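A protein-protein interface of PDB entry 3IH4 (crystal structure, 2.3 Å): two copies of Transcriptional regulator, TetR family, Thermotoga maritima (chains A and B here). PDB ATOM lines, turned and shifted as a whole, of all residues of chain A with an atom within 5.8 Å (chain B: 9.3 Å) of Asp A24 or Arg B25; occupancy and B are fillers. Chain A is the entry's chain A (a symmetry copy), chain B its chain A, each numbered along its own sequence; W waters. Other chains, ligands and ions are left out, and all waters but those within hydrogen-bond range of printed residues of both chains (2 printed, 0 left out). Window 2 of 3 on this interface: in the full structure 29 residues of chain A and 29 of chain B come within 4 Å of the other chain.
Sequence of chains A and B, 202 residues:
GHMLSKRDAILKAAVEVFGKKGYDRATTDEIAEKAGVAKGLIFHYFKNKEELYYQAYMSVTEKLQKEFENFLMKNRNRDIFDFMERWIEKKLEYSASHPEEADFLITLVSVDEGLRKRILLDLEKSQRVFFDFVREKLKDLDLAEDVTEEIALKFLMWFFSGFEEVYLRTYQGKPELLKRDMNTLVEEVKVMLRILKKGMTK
The backbone carbonyl oxygen of Ser A110 sits at hydrogen-bond distance from the guanidinium group of Arg B25. The guanidinium group (NH2) of Arg A25 sits at hydrogen-bond distance from the backbone carbonyl oxygen (O) of Ser B110. The side-chain carboxylate (OD2) of Asp B24 is in salt-bridge range of the guanidinium group (NE) of Arg A25. The guanidinium group of Arg B25 is in salt-bridge range of the side-chain carboxylate of Asp A24. The backbone NH (N) of Asp A112 sits close to the guanidinium group (NH2) of Arg B25 (3.5 Å).
The side-chain amino group (NZ) of Lys A49 is in hydrogen-bond range of the backbone carbonyl oxygen (O) of Asp A24 (3.4 Å). NH1 of Arg B25 sits at hydrogen-bond distance from O of Lys B21 (2.6 Å). The side-chain amino group (NZ) of Lys B49 lies within hydrogen-bond range of the backbone carbonyl oxygen (O) of Asp B24, at 3.4 Å. The side-chain hydroxyl of Ser B110 lies within hydrogen-bond range of the backbone carbonyl oxygen of Thr B107, 2.9 Å away. The backbone carbonyl oxygen (O) of Lys A21 sits at hydrogen-bond distance from the guanidinium group (NH1) of Arg A25 (2.6 Å).
Among the printed residues, merely in contact across the chains: Asp A24 with Asp B24 (3.9 Å), Arg A25 with Val B111 (3.8 Å) and Val A111 with Arg B25 (3.8 Å).
Of the printed residues of chain B, Asp A24 touches Asp B24 (3.9 Å) and Arg B25 (3.5 Å). Of the printed residues of chain A, Arg B25 touches Asp A24, Ser A110, Val A111 and Asp A112. Of the printed residues of chain B, Arg A25 touches Asp B24, Ser B110 and Val B111. Of the printed residues of chain B, Asp A112 touches Arg B25 (3.5 Å). Thr B107 touches none of the printed residues of chain A. Lys A49 touches none of the printed residues of chain B. The nearest printed residue of chain B that does not touch Asp A24 is Lys B21 (5.4 Å).
Of the 20 printed residues of chain B, 4 touch a printed residue of chain A. Among the printed residues, 8 pairs touch across the chains.
Asp B24 touches its own counterpart, Asp A24. Asp A24 touches Arg B25, and with the chains exchanged Arg A25 touches Asp B24. Arg A25 touches Ser B110, and with the chains exchanged Ser A110 touches Arg B25. Arg A25 touches Val B111, and with the chains exchanged Val A111 touches Arg B25. 9 positions are printed for both chains.
Water W1 lies within hydrogen-bond range of O of Lys B21, N of Arg B25, OD2 of Asp A24 and N of Asp B24. Water W2 lies within hydrogen-bond range of O of Lys A21, N of Arg A25, OD2 of Asp B24 and N of Asp A24.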
ATOM      1  N   LYS A  21       9.805  -3.263  -9.365  1.00  0.00           N
ATOM      2  CA  LYS A  21       9.802  -4.393  -8.447  1.00  0.00           C
ATOM      3  C   LYS A  21      11.018  -5.307  -8.558  1.00  0.00           C
ATOM      4  O   LYS A  21      11.340  -6.047  -7.621  1.00  0.00           O
ATOM      5  CB  LYS A  21       8.546  -5.193  -8.726  1.00  0.00           C
ATOM      6  CG  LYS A  21       7.333  -4.286  -8.792  1.00  0.00           C
ATOM      7  CD  LYS A  21       6.029  -5.005  -8.489  1.00  0.00           C
ATOM      8  CE  LYS A  21       4.863  -4.005  -8.440  1.00  0.00           C
ATOM      9  NZ  LYS A  21       4.216  -3.990  -7.117  1.00  0.00           N
ATOM     10  N   GLY A  22      11.677  -5.257  -9.716  1.00  0.00           N
ATOM     11  CA  GLY A  22      12.766  -6.142 -10.042  1.00  0.00           C
ATOM     12  C   GLY A  22      12.180  -7.382 -10.669  1.00  0.00           C
ATOM     13  O   GLY A  22      10.977  -7.607 -10.603  1.00  0.00           O
ATOM     14  N   TYR A  23      13.049  -8.200 -11.244  1.00  0.00           N
ATOM     15  CA  TYR A  23      12.662  -9.425 -11.935  1.00  0.00           C
ATOM     16  C   TYR A  23      11.844 -10.411 -11.107  1.00  0.00           C
ATOM     17  O   TYR A  23      10.774 -10.866 -11.520  1.00  0.00           O
ATOM     18  CB  TYR A  23      13.925 -10.122 -12.407  1.00  0.00           C
ATOM     19  CG  TYR A  23      13.615 -11.361 -13.137  1.00  0.00           C
ATOM     20  CD1 TYR A  23      12.998 -11.307 -14.363  1.00  0.00           C
ATOM     21  CD2 TYR A  23      13.906 -12.603 -12.601  1.00  0.00           C
ATOM     22  CE1 TYR A  23      12.692 -12.452 -15.059  1.00  0.00           C
ATOM     23  CE2 TYR A  23      13.592 -13.756 -13.295  1.00  0.00           C
ATOM     24  CZ  TYR A  23      12.978 -13.666 -14.530  1.00  0.00           C
ATOM     25  OH  TYR A  23      12.671 -14.799 -15.246  1.00  0.00           O
ATOM     26  N   ASP A  24      12.365 -10.723  -9.932  1.00  0.00           N
ATOM     27  CA  ASP A  24      11.865 -11.815  -9.111  1.00  0.00           C
ATOM     28  C   ASP A  24      10.534 -11.492  -8.498  1.00  0.00           C
ATOM     29  O   ASP A  24       9.682 -12.365  -8.397  1.00  0.00           O
ATOM     30  CB  ASP A  24      12.836 -12.134  -7.954  1.00  0.00           C
ATOM     31  CG  ASP A  24      14.087 -12.895  -8.401  1.00  0.00           C
ATOM     32  OD1 ASP A  24      14.024 -13.749  -9.318  1.00  0.00           O
ATOM     33  OD2 ASP A  24      15.146 -12.663  -7.786  1.00  0.00           O
ATOM     34  N   ARG A  25      10.378 -10.246  -8.059  1.00  0.00           N
ATOM     35  CA  ARG A  25       9.151  -9.798  -7.400  1.00  0.00           C
ATOM     36  C   ARG A  25       8.024  -9.409  -8.370  1.00  0.00           C
ATOM     37  O   ARG A  25       6.860  -9.482  -7.988  1.00  0.00           O
ATOM     38  CB  ARG A  25       9.449  -8.614  -6.467  1.00  0.00           C
ATOM     39  CG  ARG A  25       9.944  -9.012  -5.103  1.00  0.00           C
ATOM     40  CD  ARG A  25      10.219  -7.798  -4.212  1.00  0.00           C
ATOM     41  NE  ARG A  25      11.627  -7.402  -4.287  1.00  0.00           N
ATOM     42  CZ  ARG A  25      12.098  -6.225  -4.709  1.00  0.00           C
ATOM     43  NH1 ARG A  25      11.278  -5.245  -5.110  1.00  0.00           N
ATOM     44  NH2 ARG A  25      13.413  -6.023  -4.722  1.00  0.00           N
ATOM     45  N   ALA A  26       8.361  -8.972  -9.586  1.00  0.00           N
ATOM     46  CA  ALA A  26       7.349  -8.699 -10.630  1.00  0.00           C
ATOM     47  C   ALA A  26       6.619  -9.966 -11.076  1.00  0.00           C
ATOM     48  O   ALA A  26       7.196 -11.069 -11.113  1.00  0.00           O
ATOM     49  CB  ALA A  26       7.971  -8.017 -11.845  1.00  0.00           C
ATOM     50  N   LYS A  49       7.997 -15.323 -18.218  1.00  0.00           N
ATOM     51  CA  LYS A  49       8.474 -14.071 -17.633  1.00  0.00           C
ATOM     52  C   LYS A  49       9.927 -13.783 -18.016  1.00  0.00           C
ATOM     53  O   LYS A  49      10.282 -12.646 -18.267  1.00  0.00           O
ATOM     54  CB  LYS A  49       8.327 -14.060 -16.096  1.00  0.00           C
ATOM     55  CG  LYS A  49       8.787 -12.735 -15.460  1.00  0.00           C
ATOM     56  CD  LYS A  49       8.355 -12.558 -14.006  1.00  0.00           C
ATOM     57  CE  LYS A  49       8.975 -13.579 -13.083  1.00  0.00           C
ATOM     58  NZ  LYS A  49       9.241 -13.093 -11.684  1.00  0.00           N
ATOM     59  N   SER A 110      19.835  -8.032 -10.417  1.00  0.00           N
ATOM     60  CA  SER A 110      18.968  -8.880  -9.588  1.00  0.00           C
ATOM     61  C   SER A 110      18.673 -10.305 -10.145  1.00  0.00           C
ATOM     62  O   SER A 110      18.447 -11.252  -9.366  1.00  0.00           O
ATOM     63  CB  SER A 110      17.636  -8.139  -9.274  1.00  0.00           C
ATOM     64  OG  SER A 110      16.721  -8.007 -10.402  1.00  0.00           O
ATOM     65  N   VAL A 111      18.687 -10.455 -11.473  1.00  0.00           N
ATOM     66  CA  VAL A 111      18.248 -11.701 -12.130  1.00  0.00           C
ATOM     67  C   VAL A 111      19.264 -12.837 -11.982  1.00  0.00           C
ATOM     68  O   VAL A 111      20.452 -12.592 -11.784  1.00  0.00           O
ATOM     69  CB  VAL A 111      17.984 -11.480 -13.645  1.00  0.00           C
ATOM     70  CG1 VAL A 111      17.051 -10.315 -13.845  1.00  0.00           C
ATOM     71  CG2 VAL A 111      19.300 -11.242 -14.405  1.00  0.00           C
ATOM     72  N   ASP A 112      18.769 -14.074 -12.090  1.00  0.00           N
ATOM     73  CA  ASP A 112      19.599 -15.281 -12.007  1.00  0.00           C
ATOM     74  C   ASP A 112      20.683 -15.320 -13.081  1.00  0.00           C
ATOM     75  O   ASP A 112      20.503 -14.782 -14.170  1.00  0.00           O
ATOM     76  CB  ASP A 112      18.726 -16.552 -12.055  1.00  0.00           C
ATOM     77  CG  ASP A 112      18.012 -16.754 -13.404  1.00  0.00           C
ATOM     78  OD1 ASP A 112      17.000 -16.044 -13.694  1.00  0.00           O
ATOM     79  OD2 ASP A 112      18.442 -17.669 -14.157  1.00  0.00           O
ATOM     80  N   GLU A 113      21.800 -15.979 -12.775  1.00  0.00           N
ATOM     81  CA  GLU A 113      23.030 -15.824 -13.565  1.00  0.00           C
ATOM     82  C   GLU A 113      22.866 -16.263 -15.022  1.00  0.00           C
ATOM     83  O   GLU A 113      23.531 -15.730 -15.908  1.00  0.00           O
ATOM     84  CB  GLU A 113      24.224 -16.549 -12.900  1.00  0.00           C
ATOM     85  N   VAL B  17      23.161 -19.532   1.705  1.00  0.00           N
ATOM     86  CA  VAL B  17      21.974 -19.626   0.848  1.00  0.00           C
ATOM     87  C   VAL B  17      21.663 -18.290   0.222  1.00  0.00           C
ATOM     88  O   VAL B  17      21.370 -18.243  -0.969  1.00  0.00           O
ATOM     89  CB  VAL B  17      20.734 -20.162   1.595  1.00  0.00           C
ATOM     90  CG1 VAL B  17      19.482 -20.153   0.685  1.00  0.00           C
ATOM     91  CG2 VAL B  17      20.988 -21.556   2.062  1.00  0.00           C
ATOM     92  N   PHE B  18      21.764 -17.200   0.996  1.00  0.00           N
ATOM     93  CA  PHE B  18      21.562 -15.841   0.441  1.00  0.00           C
ATOM     94  C   PHE B  18      22.585 -15.541  -0.659  1.00  0.00           C
ATOM     95  O   PHE B  18      22.238 -15.063  -1.728  1.00  0.00           O
ATOM     96  CB  PHE B  18      21.617 -14.760   1.524  1.00  0.00           C
ATOM     97  CG  PHE B  18      20.360 -14.662   2.372  1.00  0.00           C
ATOM     98  CD1 PHE B  18      19.092 -14.574   1.782  1.00  0.00           C
ATOM     99  CD2 PHE B  18      20.451 -14.590   3.754  1.00  0.00           C
ATOM    100  CE1 PHE B  18      17.947 -14.475   2.563  1.00  0.00           C
ATOM    101  CE2 PHE B  18      19.314 -14.498   4.559  1.00  0.00           C
ATOM    102  CZ  PHE B  18      18.064 -14.438   3.979  1.00  0.00           C
ATOM    103  N   GLY B  19      23.845 -15.829  -0.403  1.00  0.00           N
ATOM    104  CA  GLY B  19      24.869 -15.722  -1.432  1.00  0.00           C
ATOM    105  C   GLY B  19      24.631 -16.571  -2.683  1.00  0.00           C
ATOM    106  O   GLY B  19      25.035 -16.157  -3.764  1.00  0.00           O
ATOM    107  N   LYS B  20      24.001 -17.758  -2.543  1.00  0.00           N
ATOM    108  CA  LYS B  20      23.710 -18.610  -3.714  1.00  0.00           C
ATOM    109  C   LYS B  20      22.510 -18.155  -4.513  1.00  0.00           C
ATOM    110  O   LYS B  20      22.562 -18.105  -5.730  1.00  0.00           O
ATOM    111  CB  LYS B  20      23.517 -20.072  -3.333  1.00  0.00           C
ATOM    112  CG  LYS B  20      24.835 -20.761  -3.000  1.00  0.00           C
ATOM    113  CD  LYS B  20      24.668 -22.236  -2.643  1.00  0.00           C
ATOM    114  CE  LYS B  20      23.949 -22.488  -1.286  1.00  0.00           C
ATOM    115  NZ  LYS B  20      24.030 -23.938  -0.861  1.00  0.00           N
ATOM    116  N   LYS B  21      21.429 -17.833  -3.824  1.00  0.00           N
ATOM    117  CA  LYS B  21      20.127 -17.631  -4.444  1.00  0.00           C
ATOM    118  C   LYS B  21      19.671 -16.177  -4.507  1.00  0.00           C
ATOM    119  O   LYS B  21      18.811 -15.818  -5.321  1.00  0.00           O
ATOM    120  CB  LYS B  21      19.122 -18.437  -3.647  1.00  0.00           C
ATOM    121  CG  LYS B  21      19.625 -19.849  -3.419  1.00  0.00           C
ATOM    122  CD  LYS B  21      18.509 -20.850  -3.167  1.00  0.00           C
ATOM    123  CE  LYS B  21      19.076 -22.276  -3.079  1.00  0.00           C
ATOM    124  NZ  LYS B  21      18.517 -23.148  -4.127  1.00  0.00           N
ATOM    125  N   GLY B  22      20.244 -15.351  -3.630  1.00  0.00           N
ATOM    126  CA  GLY B  22      19.841 -13.978  -3.462  1.00  0.00           C
ATOM    127  C   GLY B  22      18.728 -13.946  -2.446  1.00  0.00           C
ATOM    128  O   GLY B  22      18.161 -14.978  -2.107  1.00  0.00           O
ATOM    129  N   TYR B  23      18.397 -12.745  -1.994  1.00  0.00           N
ATOM    130  CA  TYR B  23      17.373 -12.524  -0.980  1.00  0.00           C
ATOM    131  C   TYR B  23      15.997 -13.097  -1.306  1.00  0.00           C
ATOM    132  O   TYR B  23      15.399 -13.827  -0.511  1.00  0.00           O
ATOM    133  CB  TYR B  23      17.233 -11.028  -0.765  1.00  0.00           C
ATOM    134  CG  TYR B  23      16.229 -10.723   0.266  1.00  0.00           C
ATOM    135  CD1 TYR B  23      16.463 -11.049   1.579  1.00  0.00           C
ATOM    136  CD2 TYR B  23      15.021 -10.132  -0.060  1.00  0.00           C
ATOM    137  CE1 TYR B  23      15.537 -10.780   2.558  1.00  0.00           C
ATOM    138  CE2 TYR B  23      14.084  -9.869   0.920  1.00  0.00           C
ATOM    139  CZ  TYR B  23      14.354 -10.203   2.233  1.00  0.00           C
ATOM    140  OH  TYR B  23      13.443  -9.935   3.228  1.00  0.00           O
ATOM    141  N   ASP B  24      15.515 -12.758  -2.490  1.00  0.00           N
ATOM    142  CA  ASP B  24      14.135 -13.002  -2.880  1.00  0.00           C
ATOM    143  C   ASP B  24      13.871 -14.458  -3.129  1.00  0.00           C
ATOM    144  O   ASP B  24      12.803 -14.950  -2.790  1.00  0.00           O
ATOM    145  CB  ASP B  24      13.779 -12.245  -4.178  1.00  0.00           C
ATOM    146  CG  ASP B  24      13.571 -10.742  -3.970  1.00  0.00           C
ATOM    147  OD1 ASP B  24      13.043 -10.308  -2.917  1.00  0.00           O
ATOM    148  OD2 ASP B  24      13.903  -9.986  -4.904  1.00  0.00           O
ATOM    149  N   ARG B  25      14.835 -15.130  -3.752  1.00  0.00           N
ATOM    150  CA  ARG B  25      14.701 -16.545  -4.099  1.00  0.00           C
ATOM    151  C   ARG B  25      15.022 -17.506  -2.945  1.00  0.00           C
ATOM    152  O   ARG B  25      14.512 -18.623  -2.944  1.00  0.00           O
ATOM    153  CB  ARG B  25      15.592 -16.883  -5.305  1.00  0.00           C
ATOM    154  CG  ARG B  25      14.969 -16.577  -6.640  1.00  0.00           C
ATOM    155  CD  ARG B  25      15.893 -16.938  -7.805  1.00  0.00           C
ATOM    156  NE  ARG B  25      16.677 -15.776  -8.231  1.00  0.00           N
ATOM    157  CZ  ARG B  25      18.009 -15.672  -8.223  1.00  0.00           C
ATOM    158  NH1 ARG B  25      18.787 -16.681  -7.812  1.00  0.00           N
ATOM    159  NH2 ARG B  25      18.570 -14.540  -8.639  1.00  0.00           N
ATOM    160  N   ALA B  26      15.874 -17.098  -2.001  1.00  0.00           N
ATOM    161  CA  ALA B  26      16.142 -17.900  -0.787  1.00  0.00           C
ATOM    162  C   ALA B  26      14.910 -18.028   0.108  1.00  0.00           C
ATOM    163  O   ALA B  26      14.078 -17.107   0.204  1.00  0.00           O
ATOM    164  CB  ALA B  26      17.298 -17.318   0.021  1.00  0.00           C
ATOM    165  N   THR B  27      14.799 -19.192   0.750  1.00  0.00           N
ATOM    166  CA  THR B  27      13.764 -19.466   1.725  1.00  0.00           C
ATOM    167  C   THR B  27      14.431 -19.733   3.057  1.00  0.00           C
ATOM    168  O   THR B  27      15.501 -20.349   3.117  1.00  0.00           O
ATOM    169  CB  THR B  27      12.926 -20.726   1.356  1.00  0.00           C
ATOM    170  OG1 THR B  27      13.684 -21.912   1.609  1.00  0.00           O
ATOM    171  CG2 THR B  27      12.489 -20.712  -0.123  1.00  0.00           C
ATOM    172  N   THR B  28      13.780 -19.299   4.126  1.00  0.00           N
ATOM    173  CA  THR B  28      14.186 -19.658   5.469  1.00  0.00           C
ATOM    174  C   THR B  28      14.033 -21.192   5.729  1.00  0.00           C
ATOM    175  O   THR B  28      14.710 -21.751   6.588  1.00  0.00           O
ATOM    176  CB  THR B  28      13.376 -18.847   6.507  1.00  0.00           C
ATOM    177  OG1 THR B  28      12.021 -19.278   6.480  1.00  0.00           O
ATOM    178  CG2 THR B  28      13.414 -17.354   6.193  1.00  0.00           C
ATOM    179  N   ASP B  29      13.132 -21.854   4.998  1.00  0.00           N
ATOM    180  CA  ASP B  29      12.982 -23.294   5.111  1.00  0.00           C
ATOM    181  C   ASP B  29      14.284 -23.999   4.698  1.00  0.00           C
ATOM    182  O   ASP B  29      14.698 -24.952   5.345  1.00  0.00           O
ATOM    183  CB  ASP B  29      11.840 -23.824   4.250  1.00  0.00           C
ATOM    184  CG  ASP B  29      10.494 -23.160   4.551  1.00  0.00           C
ATOM    185  OD1 ASP B  29      10.236 -22.025   4.043  1.00  0.00           O
ATOM    186  OD2 ASP B  29       9.683 -23.793   5.261  1.00  0.00           O
ATOM    187  N   GLU B  30      14.931 -23.544   3.627  1.00  0.00           N
ATOM    188  CA  GLU B  30      16.159 -24.201   3.186  1.00  0.00           C
ATOM    189  C   GLU B  30      17.364 -23.747   3.973  1.00  0.00           C
ATOM    190  O   GLU B  30      18.315 -24.486   4.083  1.00  0.00           O
ATOM    191  CB  GLU B  30      16.391 -24.038   1.683  1.00  0.00           C
ATOM    192  CG  GLU B  30      16.878 -22.708   1.229  1.00  0.00           C
ATOM    193  CD  GLU B  30      16.498 -22.411  -0.225  1.00  0.00           C
ATOM    194  OE1 GLU B  30      16.882 -23.215  -1.097  1.00  0.00           O
ATOM    195  OE2 GLU B  30      15.823 -21.378  -0.492  1.00  0.00           O
ATOM    196  N   ILE B  31      17.330 -22.535   4.518  1.00  0.00           N
ATOM    197  CA  ILE B  31      18.356 -22.074   5.464  1.00  0.00           C
ATOM    198  C   ILE B  31      18.335 -22.958   6.716  1.00  0.00           C
ATOM    199  O   ILE B  31      19.380 -23.392   7.191  1.00  0.00           O
ATOM    200  CB  ILE B  31      18.184 -20.551   5.804  1.00  0.00           C
ATOM    201  CG1 ILE B  31      18.527 -19.690   4.573  1.00  0.00           C
ATOM    202  CG2 ILE B  31      19.032 -20.147   7.035  1.00  0.00           C
ATOM    203  CD1 ILE B  31      18.314 -18.215   4.742  1.00  0.00           C
ATOM    204  N   LYS B  49      12.511 -13.397   7.484  1.00  0.00           N
ATOM    205  CA  LYS B  49      13.617 -13.523   6.537  1.00  0.00           C
ATOM    206  C   LYS B  49      14.406 -12.218   6.407  1.00  0.00           C
ATOM    207  O   LYS B  49      15.618 -12.241   6.298  1.00  0.00           O
ATOM    208  CB  LYS B  49      13.134 -13.982   5.144  1.00  0.00           C
ATOM    209  CG  LYS B  49      14.286 -14.161   4.138  1.00  0.00           C
ATOM    210  CD  LYS B  49      13.898 -14.921   2.873  1.00  0.00           C
ATOM    211  CE  LYS B  49      12.871 -14.189   2.043  1.00  0.00           C
ATOM    212  NZ  LYS B  49      12.979 -14.409   0.558  1.00  0.00           N
ATOM    213  N   THR B 107      24.945  -9.375  -2.700  1.00  0.00           N
ATOM    214  CA  THR B 107      23.502  -9.500  -2.844  1.00  0.00           C
ATOM    215  C   THR B 107      22.743  -8.264  -2.372  1.00  0.00           C
ATOM    216  O   THR B 107      21.539  -8.156  -2.609  1.00  0.00           O
ATOM    217  CB  THR B 107      22.936 -10.722  -2.071  1.00  0.00           C
ATOM    218  OG1 THR B 107      23.265 -10.619  -0.673  1.00  0.00           O
ATOM    219  CG2 THR B 107      23.503 -11.994  -2.669  1.00  0.00           C
ATOM    220  N   SER B 110      20.234  -6.783  -4.796  1.00  0.00           N
ATOM    221  CA  SER B 110      18.971  -7.451  -5.137  1.00  0.00           C
ATOM    222  C   SER B 110      17.751  -7.102  -4.232  1.00  0.00           C
ATOM    223  O   SER B 110      16.592  -7.139  -4.695  1.00  0.00           O
ATOM    224  CB  SER B 110      19.176  -8.992  -5.193  1.00  0.00           C
ATOM    225  OG  SER B 110      19.368  -9.638  -3.899  1.00  0.00           O
ATOM    226  N   VAL B 111      18.007  -6.759  -2.967  1.00  0.00           N
ATOM    227  CA  VAL B 111      16.939  -6.585  -1.964  1.00  0.00           C
ATOM    228  C   VAL B 111      16.148  -5.290  -2.163  1.00  0.00           C
ATOM    229  O   VAL B 111      16.650  -4.333  -2.749  1.00  0.00           O
ATOM    230  CB  VAL B 111      17.511  -6.587  -0.520  1.00  0.00           C
ATOM    231  CG1 VAL B 111      18.369  -7.807  -0.302  1.00  0.00           C
ATOM    232  CG2 VAL B 111      18.326  -5.311  -0.247  1.00  0.00           C
ATOM    233  N   GLN B 172      32.398 -13.880  -8.781  1.00  0.00           N
ATOM    234  CA  GLN B 172      31.343 -14.512  -8.006  1.00  0.00           C
ATOM    235  C   GLN B 172      31.308 -15.983  -8.415  1.00  0.00           C
ATOM    236  O   GLN B 172      31.204 -16.312  -9.606  1.00  0.00           O
ATOM    237  CB  GLN B 172      29.987 -13.805  -8.261  1.00  0.00           C
ATOM    238  CG  GLN B 172      28.707 -14.482  -7.709  1.00  0.00           C
ATOM    239  CD  GLN B 172      27.418 -13.958  -8.388  1.00  0.00           C
ATOM    240  OE1 GLN B 172      27.357 -13.763  -9.611  1.00  0.00           O
ATOM    241  NE2 GLN B 172      26.385 -13.735  -7.586  1.00  0.00           N
HETATM  242  O   HOH W   1      16.937 -13.636  -5.381  1.00  0.00           O
HETATM  243  O   HOH W   2      12.817  -8.511  -7.470  1.00  0.00           O
